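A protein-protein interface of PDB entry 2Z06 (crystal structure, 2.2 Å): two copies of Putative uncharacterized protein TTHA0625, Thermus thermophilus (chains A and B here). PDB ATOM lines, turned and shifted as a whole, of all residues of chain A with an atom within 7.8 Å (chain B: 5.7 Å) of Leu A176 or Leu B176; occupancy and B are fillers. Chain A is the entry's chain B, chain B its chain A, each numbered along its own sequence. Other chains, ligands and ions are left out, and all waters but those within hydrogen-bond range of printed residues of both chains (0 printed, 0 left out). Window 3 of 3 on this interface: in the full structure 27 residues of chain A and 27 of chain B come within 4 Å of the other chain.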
ATOM      1  N   VAL A 173      28.648  20.202  24.469  1.00  0.00           N
ATOM      2  CA  VAL A 173      27.850  20.000  23.263  1.00  0.00           C
ATOM      3  C   VAL A 173      27.736  18.500  23.045  1.00  0.00           C
ATOM      4  O   VAL A 173      28.732  17.797  23.065  1.00  0.00           O
ATOM      5  CB  VAL A 173      28.505  20.654  22.026  1.00  0.00           C
ATOM      6  CG1 VAL A 173      27.602  20.478  20.801  1.00  0.00           C
ATOM      7  CG2 VAL A 173      28.749  22.148  22.287  1.00  0.00           C
ATOM      8  N   PRO A 174      26.510  17.985  22.876  1.00  0.00           N
ATOM      9  CA  PRO A 174      26.313  16.549  22.665  1.00  0.00           C
ATOM     10  C   PRO A 174      26.837  16.115  21.305  1.00  0.00           C
ATOM     11  O   PRO A 174      26.593  16.795  20.295  1.00  0.00           O
ATOM     12  CB  PRO A 174      24.802  16.395  22.786  1.00  0.00           C
ATOM     13  CG  PRO A 174      24.306  17.695  22.197  1.00  0.00           C
ATOM     14  CD  PRO A 174      25.223  18.701  22.848  1.00  0.00           C
ATOM     15  N   THR A 175      27.559  14.994  21.274  1.00  0.00           N
ATOM     16  CA  THR A 175      28.114  14.497  20.017  1.00  0.00           C
ATOM     17  C   THR A 175      27.270  13.391  19.400  1.00  0.00           C
ATOM     18  O   THR A 175      26.617  12.621  20.110  1.00  0.00           O
ATOM     19  CB  THR A 175      29.558  13.972  20.198  1.00  0.00           C
ATOM     20  OG1 THR A 175      29.593  12.990  21.244  1.00  0.00           O
ATOM     21  CG2 THR A 175      30.500  15.120  20.547  1.00  0.00           C
ATOM     22  N   LEU A 176      27.278  13.326  18.074  1.00  0.00           N
ATOM     23  CA  LEU A 176      26.525  12.304  17.344  1.00  0.00           C
ATOM     24  C   LEU A 176      27.457  11.136  17.036  1.00  0.00           C
ATOM     25  O   LEU A 176      27.598  10.737  15.876  1.00  0.00           O
ATOM     26  CB  LEU A 176      25.992  12.880  16.027  1.00  0.00           C
ATOM     27  CG  LEU A 176      24.787  12.257  15.300  1.00  0.00           C
ATOM     28  CD1 LEU A 176      24.795  10.746  15.434  1.00  0.00           C
ATOM     29  CD2 LEU A 176      23.500  12.825  15.882  1.00  0.00           C
ATOM     30  N   ASP A 177      28.095  10.583  18.061  1.00  0.00           N
ATOM     31  CA  ASP A 177      29.013   9.467  17.831  1.00  0.00           C
ATOM     32  C   ASP A 177      28.882   8.295  18.799  1.00  0.00           C
ATOM     33  O   ASP A 177      29.852   7.567  19.027  1.00  0.00           O
ATOM     34  CB  ASP A 177      30.464   9.960  17.839  1.00  0.00           C
ATOM     35  CG  ASP A 177      30.945  10.370  19.225  1.00  0.00           C
ATOM     36  OD1 ASP A 177      32.165  10.571  19.380  1.00  0.00           O
ATOM     37  OD2 ASP A 177      30.125  10.501  20.149  1.00  0.00           O
ATOM     38  N   ALA A 178      27.694   8.116  19.367  1.00  0.00           N
ATOM     39  CA  ALA A 178      27.452   7.010  20.290  1.00  0.00           C
ATOM     40  C   ALA A 178      27.692   5.708  19.530  1.00  0.00           C
ATOM     41  O   ALA A 178      27.091   5.486  18.479  1.00  0.00           O
ATOM     42  CB  ALA A 178      26.023   7.058  20.805  1.00  0.00           C
ATOM     43  N   THR A 179      28.575   4.861  20.057  1.00  0.00           N
ATOM     44  CA  THR A 179      28.903   3.587  19.416  1.00  0.00           C
ATOM     45  C   THR A 179      29.511   2.627  20.415  1.00  0.00           C
ATOM     46  O   THR A 179      29.640   2.932  21.601  1.00  0.00           O
ATOM     47  CB  THR A 179      29.959   3.741  18.301  1.00  0.00           C
ATOM     48  OG1 THR A 179      31.124   4.386  18.838  1.00  0.00           O
ATOM     49  CG2 THR A 179      29.413   4.544  17.132  1.00  0.00           C
ATOM     50  N   TYR A 187      30.631   4.015  23.923  1.00  0.00           N
ATOM     51  CA  TYR A 187      31.309   5.300  23.994  1.00  0.00           C
ATOM     52  C   TYR A 187      30.603   6.461  23.300  1.00  0.00           C
ATOM     53  O   TYR A 187      29.903   6.285  22.310  1.00  0.00           O
ATOM     54  CB  TYR A 187      32.724   5.140  23.422  1.00  0.00           C
ATOM     55  CG  TYR A 187      33.462   6.440  23.175  1.00  0.00           C
ATOM     56  CD1 TYR A 187      33.476   7.028  21.912  1.00  0.00           C
ATOM     57  CD2 TYR A 187      34.111   7.102  24.215  1.00  0.00           C
ATOM     58  CE1 TYR A 187      34.112   8.249  21.692  1.00  0.00           C
ATOM     59  CE2 TYR A 187      34.749   8.317  24.004  1.00  0.00           C
ATOM     60  CZ  TYR A 187      34.748   8.890  22.748  1.00  0.00           C
ATOM     61  OH  TYR A 187      35.380  10.102  22.549  1.00  0.00           O
ATOM     62  N   GLN A 188      30.786   7.650  23.856  1.00  0.00           N
ATOM     63  CA  GLN A 188      30.247   8.885  23.284  1.00  0.00           C
ATOM     64  C   GLN A 188      31.226   9.973  23.729  1.00  0.00           C
ATOM     65  O   GLN A 188      31.608  10.025  24.897  1.00  0.00           O
ATOM     66  CB  GLN A 188      28.833   9.189  23.807  1.00  0.00           C
ATOM     67  CG  GLN A 188      28.141  10.328  23.045  1.00  0.00           C
ATOM     68  CD  GLN A 188      26.843  10.810  23.703  1.00  0.00           C
ATOM     69  OE1 GLN A 188      26.069  11.555  23.099  1.00  0.00           O
ATOM     70  NE2 GLN A 188      26.611  10.397  24.939  1.00  0.00           N
ATOM     71  N   THR A 189      31.642  10.829  22.801  1.00  0.00           N
ATOM     72  CA  THR A 189      32.597  11.885  23.122  1.00  0.00           C
ATOM     73  C   THR A 189      32.072  12.900  24.131  1.00  0.00           C
ATOM     74  O   THR A 189      32.785  13.280  25.053  1.00  0.00           O
ATOM     75  CB  THR A 189      33.057  12.601  21.853  1.00  0.00           C
ATOM     76  OG1 THR A 189      33.635  11.629  20.974  1.00  0.00           O
ATOM     77  CG2 THR A 189      34.098  13.692  22.187  1.00  0.00           C
ATOM     78  N   ASP A 190      30.843  13.362  23.956  1.00  0.00           N
ATOM     79  CA  ASP A 190      30.285  14.283  24.936  1.00  0.00           C
ATOM     80  C   ASP A 190      28.785  14.082  25.040  1.00  0.00           C
ATOM     81  O   ASP A 190      28.092  13.970  24.036  1.00  0.00           O
ATOM     82  CB  ASP A 190      30.597  15.743  24.606  1.00  0.00           C
ATOM     83  CG  ASP A 190      30.814  16.581  25.863  1.00  0.00           C
ATOM     84  OD1 ASP A 190      31.974  16.706  26.304  1.00  0.00           O
ATOM     85  OD2 ASP A 190      29.826  17.098  26.435  1.00  0.00           O
ATOM     86  N   TYR A 197      20.310  26.552  26.215  1.00  0.00           N
ATOM     87  CA  TYR A 197      21.224  26.683  25.091  1.00  0.00           C
ATOM     88  C   TYR A 197      21.117  28.070  24.485  1.00  0.00           C
ATOM     89  O   TYR A 197      21.758  28.374  23.483  1.00  0.00           O
ATOM     90  CB  TYR A 197      20.976  25.601  24.033  1.00  0.00           C
ATOM     91  CG  TYR A 197      21.659  24.289  24.376  1.00  0.00           C
ATOM     92  CD1 TYR A 197      21.284  23.554  25.508  1.00  0.00           C
ATOM     93  CD2 TYR A 197      22.714  23.806  23.603  1.00  0.00           C
ATOM     94  CE1 TYR A 197      21.944  22.377  25.862  1.00  0.00           C
ATOM     95  CE2 TYR A 197      23.382  22.628  23.947  1.00  0.00           C
ATOM     96  CZ  TYR A 197      22.994  21.920  25.081  1.00  0.00           C
ATOM     97  OH  TYR A 197      23.665  20.765  25.434  1.00  0.00           O
ATOM     98  N   ARG A 228      17.377  22.630  27.931  1.00  0.00           N
ATOM     99  CA  ARG A 228      17.327  21.370  27.199  1.00  0.00           C
ATOM    100  C   ARG A 228      17.943  20.360  28.160  1.00  0.00           C
ATOM    101  O   ARG A 228      18.964  20.633  28.799  1.00  0.00           O
ATOM    102  CB  ARG A 228      18.152  21.417  25.902  1.00  0.00           C
ATOM    103  CG  ARG A 228      17.375  21.806  24.646  1.00  0.00           C
ATOM    104  CD  ARG A 228      17.984  21.151  23.389  1.00  0.00           C
ATOM    105  NE  ARG A 228      19.344  21.601  23.073  1.00  0.00           N
ATOM    106  CZ  ARG A 228      20.154  20.996  22.205  1.00  0.00           C
ATOM    107  NH1 ARG A 228      21.372  21.474  21.971  1.00  0.00           N
ATOM    108  NH2 ARG A 228      19.755  19.898  21.581  1.00  0.00           N
ATOM    109  N   HIS A 230      19.853  17.058  28.572  1.00  0.00           N
ATOM    110  CA  HIS A 230      20.720  16.194  27.777  1.00  0.00           C
ATOM    111  C   HIS A 230      21.291  15.062  28.607  1.00  0.00           C
ATOM    112  O   HIS A 230      21.855  15.271  29.681  1.00  0.00           O
ATOM    113  CB  HIS A 230      21.848  17.008  27.140  1.00  0.00           C
ATOM    114  CG  HIS A 230      21.430  17.741  25.902  1.00  0.00           C
ATOM    115  ND1 HIS A 230      21.196  17.104  24.702  1.00  0.00           N
ATOM    116  CD2 HIS A 230      21.187  19.055  25.683  1.00  0.00           C
ATOM    117  CE1 HIS A 230      20.833  17.995  23.796  1.00  0.00           C
ATOM    118  NE2 HIS A 230      20.819  19.186  24.366  1.00  0.00           N
ATOM    119  N   PRO A 246      21.710   8.359  23.155  1.00  0.00           N
ATOM    120  CA  PRO A 246      21.612   9.742  23.619  1.00  0.00           C
ATOM    121  C   PRO A 246      20.139  10.089  23.865  1.00  0.00           C
ATOM    122  O   PRO A 246      19.252   9.555  23.202  1.00  0.00           O
ATOM    123  CB  PRO A 246      22.224  10.534  22.464  1.00  0.00           C
ATOM    124  CG  PRO A 246      23.226   9.567  21.889  1.00  0.00           C
ATOM    125  CD  PRO A 246      22.439   8.279  21.879  1.00  0.00           C
ATOM    126  N   TYR A 247      19.886  10.976  24.820  1.00  0.00           N
ATOM    127  CA  TYR A 247      18.525  11.370  25.155  1.00  0.00           C
ATOM    128  C   TYR A 247      18.400  12.876  25.293  1.00  0.00           C
ATOM    129  O   TYR A 247      19.248  13.523  25.911  1.00  0.00           O
ATOM    130  CB  TYR A 247      18.092  10.705  26.463  1.00  0.00           C
ATOM    131  CG  TYR A 247      16.687  11.060  26.900  1.00  0.00           C
ATOM    132  CD1 TYR A 247      16.420  12.255  27.572  1.00  0.00           C
ATOM    133  CD2 TYR A 247      15.620  10.202  26.635  1.00  0.00           C
ATOM    134  CE1 TYR A 247      15.121  12.584  27.969  1.00  0.00           C
ATOM    135  CE2 TYR A 247      14.320  10.520  27.025  1.00  0.00           C
ATOM    136  CZ  TYR A 247      14.073  11.710  27.691  1.00  0.00           C
ATOM    137  OH  TYR A 247      12.781  12.022  28.070  1.00  0.00           O
ATOM    138  N   VAL A 248      17.327  13.424  24.728  1.00  0.00           N
ATOM    139  CA  VAL A 248      17.077  14.855  24.784  1.00  0.00           C
ATOM    140  C   VAL A 248      15.628  15.176  25.144  1.00  0.00           C
ATOM    141  O   VAL A 248      14.702  14.502  24.695  1.00  0.00           O
ATOM    142  CB  VAL A 248      17.364  15.532  23.432  1.00  0.00           C
ATOM    143  CG1 VAL A 248      17.317  17.038  23.599  1.00  0.00           C
ATOM    144  CG2 VAL A 248      18.707  15.091  22.896  1.00  0.00           C
ATOM    145  N   VAL B 173      34.507  15.291  15.492  1.00  0.00           N
ATOM    146  CA  VAL B 173      33.363  14.530  15.971  1.00  0.00           C
ATOM    147  C   VAL B 173      32.097  15.324  15.672  1.00  0.00           C
ATOM    148  O   VAL B 173      31.975  16.472  16.080  1.00  0.00           O
ATOM    149  CB  VAL B 173      33.461  14.266  17.494  1.00  0.00           C
ATOM    150  CG1 VAL B 173      32.237  13.505  17.977  1.00  0.00           C
ATOM    151  CG2 VAL B 173      34.708  13.467  17.793  1.00  0.00           C
ATOM    152  N   PRO B 174      31.148  14.728  14.933  1.00  0.00           N
ATOM    153  CA  PRO B 174      29.910  15.447  14.616  1.00  0.00           C
ATOM    154  C   PRO B 174      29.112  15.777  15.881  1.00  0.00           C
ATOM    155  O   PRO B 174      28.939  14.926  16.757  1.00  0.00           O
ATOM    156  CB  PRO B 174      29.170  14.475  13.689  1.00  0.00           C
ATOM    157  CG  PRO B 174      29.642  13.122  14.165  1.00  0.00           C
ATOM    158  CD  PRO B 174      31.124  13.358  14.388  1.00  0.00           C
ATOM    159  N   THR B 175      28.650  17.021  15.984  1.00  0.00           N
ATOM    160  CA  THR B 175      27.861  17.447  17.142  1.00  0.00           C
ATOM    161  C   THR B 175      26.387  17.488  16.759  1.00  0.00           C
ATOM    162  O   THR B 175      26.044  17.770  15.609  1.00  0.00           O
ATOM    163  CB  THR B 175      28.261  18.846  17.627  1.00  0.00           C
ATOM    164  OG1 THR B 175      28.239  19.753  16.520  1.00  0.00           O
ATOM    165  CG2 THR B 175      29.636  18.832  18.240  1.00  0.00           C
ATOM    166  N   LEU B 176      25.517  17.200  17.719  1.00  0.00           N
ATOM    167  CA  LEU B 176      24.088  17.217  17.458  1.00  0.00           C
ATOM    168  C   LEU B 176      23.477  18.483  18.047  1.00  0.00           C
ATOM    169  O   LEU B 176      22.753  18.446  19.042  1.00  0.00           O
ATOM    170  CB  LEU B 176      23.428  15.967  18.049  1.00  0.00           C
ATOM    171  CG  LEU B 176      21.924  15.783  17.791  1.00  0.00           C
ATOM    172  CD1 LEU B 176      21.576  16.019  16.316  1.00  0.00           C
ATOM    173  CD2 LEU B 176      21.532  14.385  18.220  1.00  0.00           C
ATOM    174  N   ASP B 177      23.790  19.610  17.421  1.00  0.00           N
ATOM    175  CA  ASP B 177      23.281  20.891  17.870  1.00  0.00           C
ATOM    176  C   ASP B 177      23.034  21.814  16.688  1.00  0.00           C
ATOM    177  O   ASP B 177      23.100  23.036  16.818  1.00  0.00           O
ATOM    178  CB  ASP B 177      24.263  21.547  18.850  1.00  0.00           C
ATOM    179  CG  ASP B 177      25.587  21.933  18.200  1.00  0.00           C
ATOM    180  OD1 ASP B 177      26.348  22.691  18.830  1.00  0.00           O
ATOM    181  OD2 ASP B 177      25.874  21.478  17.074  1.00  0.00           O
ATOM    182  N   ALA B 178      22.763  21.228  15.528  1.00  0.00           N
ATOM    183  CA  ALA B 178      22.484  22.028  14.341  1.00  0.00           C
ATOM    184  C   ALA B 178      21.245  22.826  14.712  1.00  0.00           C
ATOM    185  O   ALA B 178      20.213  22.257  15.072  1.00  0.00           O
ATOM    186  CB  ALA B 178      22.208  21.134  13.146  1.00  0.00           C
ATOM    187  N   GLN B 188      26.257  24.884  13.648  1.00  0.00           N
ATOM    188  CA  GLN B 188      26.568  23.532  14.106  1.00  0.00           C
ATOM    189  C   GLN B 188      27.998  23.594  14.647  1.00  0.00           C
ATOM    190  O   GLN B 188      28.911  24.032  13.944  1.00  0.00           O
ATOM    191  CB  GLN B 188      26.495  22.507  12.974  1.00  0.00           C
ATOM    192  CG  GLN B 188      26.790  21.075  13.469  1.00  0.00           C
ATOM    193  CD  GLN B 188      26.929  20.054  12.343  1.00  0.00           C
ATOM    194  OE1 GLN B 188      26.883  18.841  12.578  1.00  0.00           O
ATOM    195  NE2 GLN B 188      27.107  20.539  11.125  1.00  0.00           N
ATOM    196  N   HIS B 230      31.073  12.262   6.599  1.00  0.00           N
ATOM    197  CA  HIS B 230      30.379  13.214   7.449  1.00  0.00           C
ATOM    198  C   HIS B 230      30.256  14.568   6.783  1.00  0.00           C
ATOM    199  O   HIS B 230      31.246  15.166   6.389  1.00  0.00           O
ATOM    200  CB  HIS B 230      31.107  13.355   8.792  1.00  0.00           C
ATOM    201  CG  HIS B 230      30.749  12.299   9.788  1.00  0.00           C
ATOM    202  ND1 HIS B 230      29.519  12.250  10.409  1.00  0.00           N
ATOM    203  CD2 HIS B 230      31.462  11.260  10.283  1.00  0.00           C
ATOM    204  CE1 HIS B 230      29.492  11.228  11.245  1.00  0.00           C
ATOM    205  NE2 HIS B 230      30.659  10.610  11.188  1.00  0.00           N
ATOM    206  N   PRO B 246      22.613  17.650   9.390  1.00  0.00           N
ATOM    207  CA  PRO B 246      23.780  16.775   9.493  1.00  0.00           C
ATOM    208  C   PRO B 246      23.550  15.566   8.599  1.00  0.00           C
ATOM    209  O   PRO B 246      22.472  14.968   8.623  1.00  0.00           O
ATOM    210  CB  PRO B 246      23.796  16.404  10.970  1.00  0.00           C
ATOM    211  CG  PRO B 246      23.243  17.627  11.617  1.00  0.00           C
ATOM    212  CD  PRO B 246      22.073  17.953  10.728  1.00  0.00           C
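The backbone carbonyl oxygen (O) of Pro B174 is in hydrogen-bond range of the backbone NH (N) of Leu A176 (2.7 Å). N of Leu B176 lies within hydrogen-bond range of O of Pro A174 (2.8 Å).
OG1 of Thr B175 is in hydrogen-bond range of OD2 of Asp B177, at 3.0 Å. OG1 of Thr A175 sits at hydrogen-bond distance from OD2 of Asp A177. O of Thr A175 lies close to OE1 of Gln A188 (3.2 Å). OG1 of Thr A175 is in hydrogen-bond range of N of Thr A189, 3.4 Å away. The side-chain hydroxyl of Thr A179 is in hydrogen-bond range of the backbone carbonyl oxygen of Asp A177. OD1 of Asp A177 is in hydrogen-bond range of OG1 of Thr A189, at 2.4 Å.
Among the printed residues, pairs that only touch across the chains: Val A173 with Asp B177 (3.2 Å), Asp A177 with Val B173 (3.3 Å), Thr A175 with Pro B174 (3.4 Å), Leu A176 with Leu B176 (3.4 Å), Pro A174 with Thr B175 (3.5 Å), Thr A175 with Val B173 (3.5 Å), Val A173 with Thr B175 (3.6 Å) and Thr A189 with Val B173 (3.8 Å).
Of chain B, only Pro B174 and Leu B176 come within 4 Å of Leu A176. Of chain A, only Pro A174 and Leu A176 come within 4 Å of Leu B176. Of the printed residues of chain B, Thr A189 touches Val B173 (3.8 Å). Of the printed residues of chain B, Asp A177 touches Val B173. Of the printed residues of chain A, Thr B175 touches Val A173 and Pro A174. Gln B188 touches none of the printed residues of chain A. Val A248 touches none of the printed residues of chain B. The nearest residue of chain B that does not touch Leu A176 is Thr B175 (4.3 Å). The nearest printed residue of chain B that does not touch Pro A174 is Pro B174 (4.6 Å).
Hydrophobic or aromatic side chains of chain B that line the printed part of chain A: Val B173, Pro B174 and Leu B176. Of the 17 printed residues of chain A, 6 touch a printed residue of chain B. Hydrophobic or aromatic side chains of chain A that line the printed part of chain B: Val A173, Pro A174 and Leu A176. Among the printed residues, no Asp or Glu carboxylate lies within 4 Å of a Lys or Arg side-chain nitrogen of the other chain.
Val A173 touches Asp B177, and with the chains exchanged Asp A177 touches Val B173. Pro A174 touches Thr B175, and with the chains exchanged Thr A175 touches Pro B174. Pro A174 touches Leu B176, and with the chains exchanged Leu A176 touches Pro B174. Leu A176 touches its own counterpart, Leu B176. Positions printed for both chains: 173, 174, 175, 176, 177, 178, 188, 230 and 246. Of the 10 pairs that touch across the chains among the printed residues, 9 have their exchanged pair printed and touching as well.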
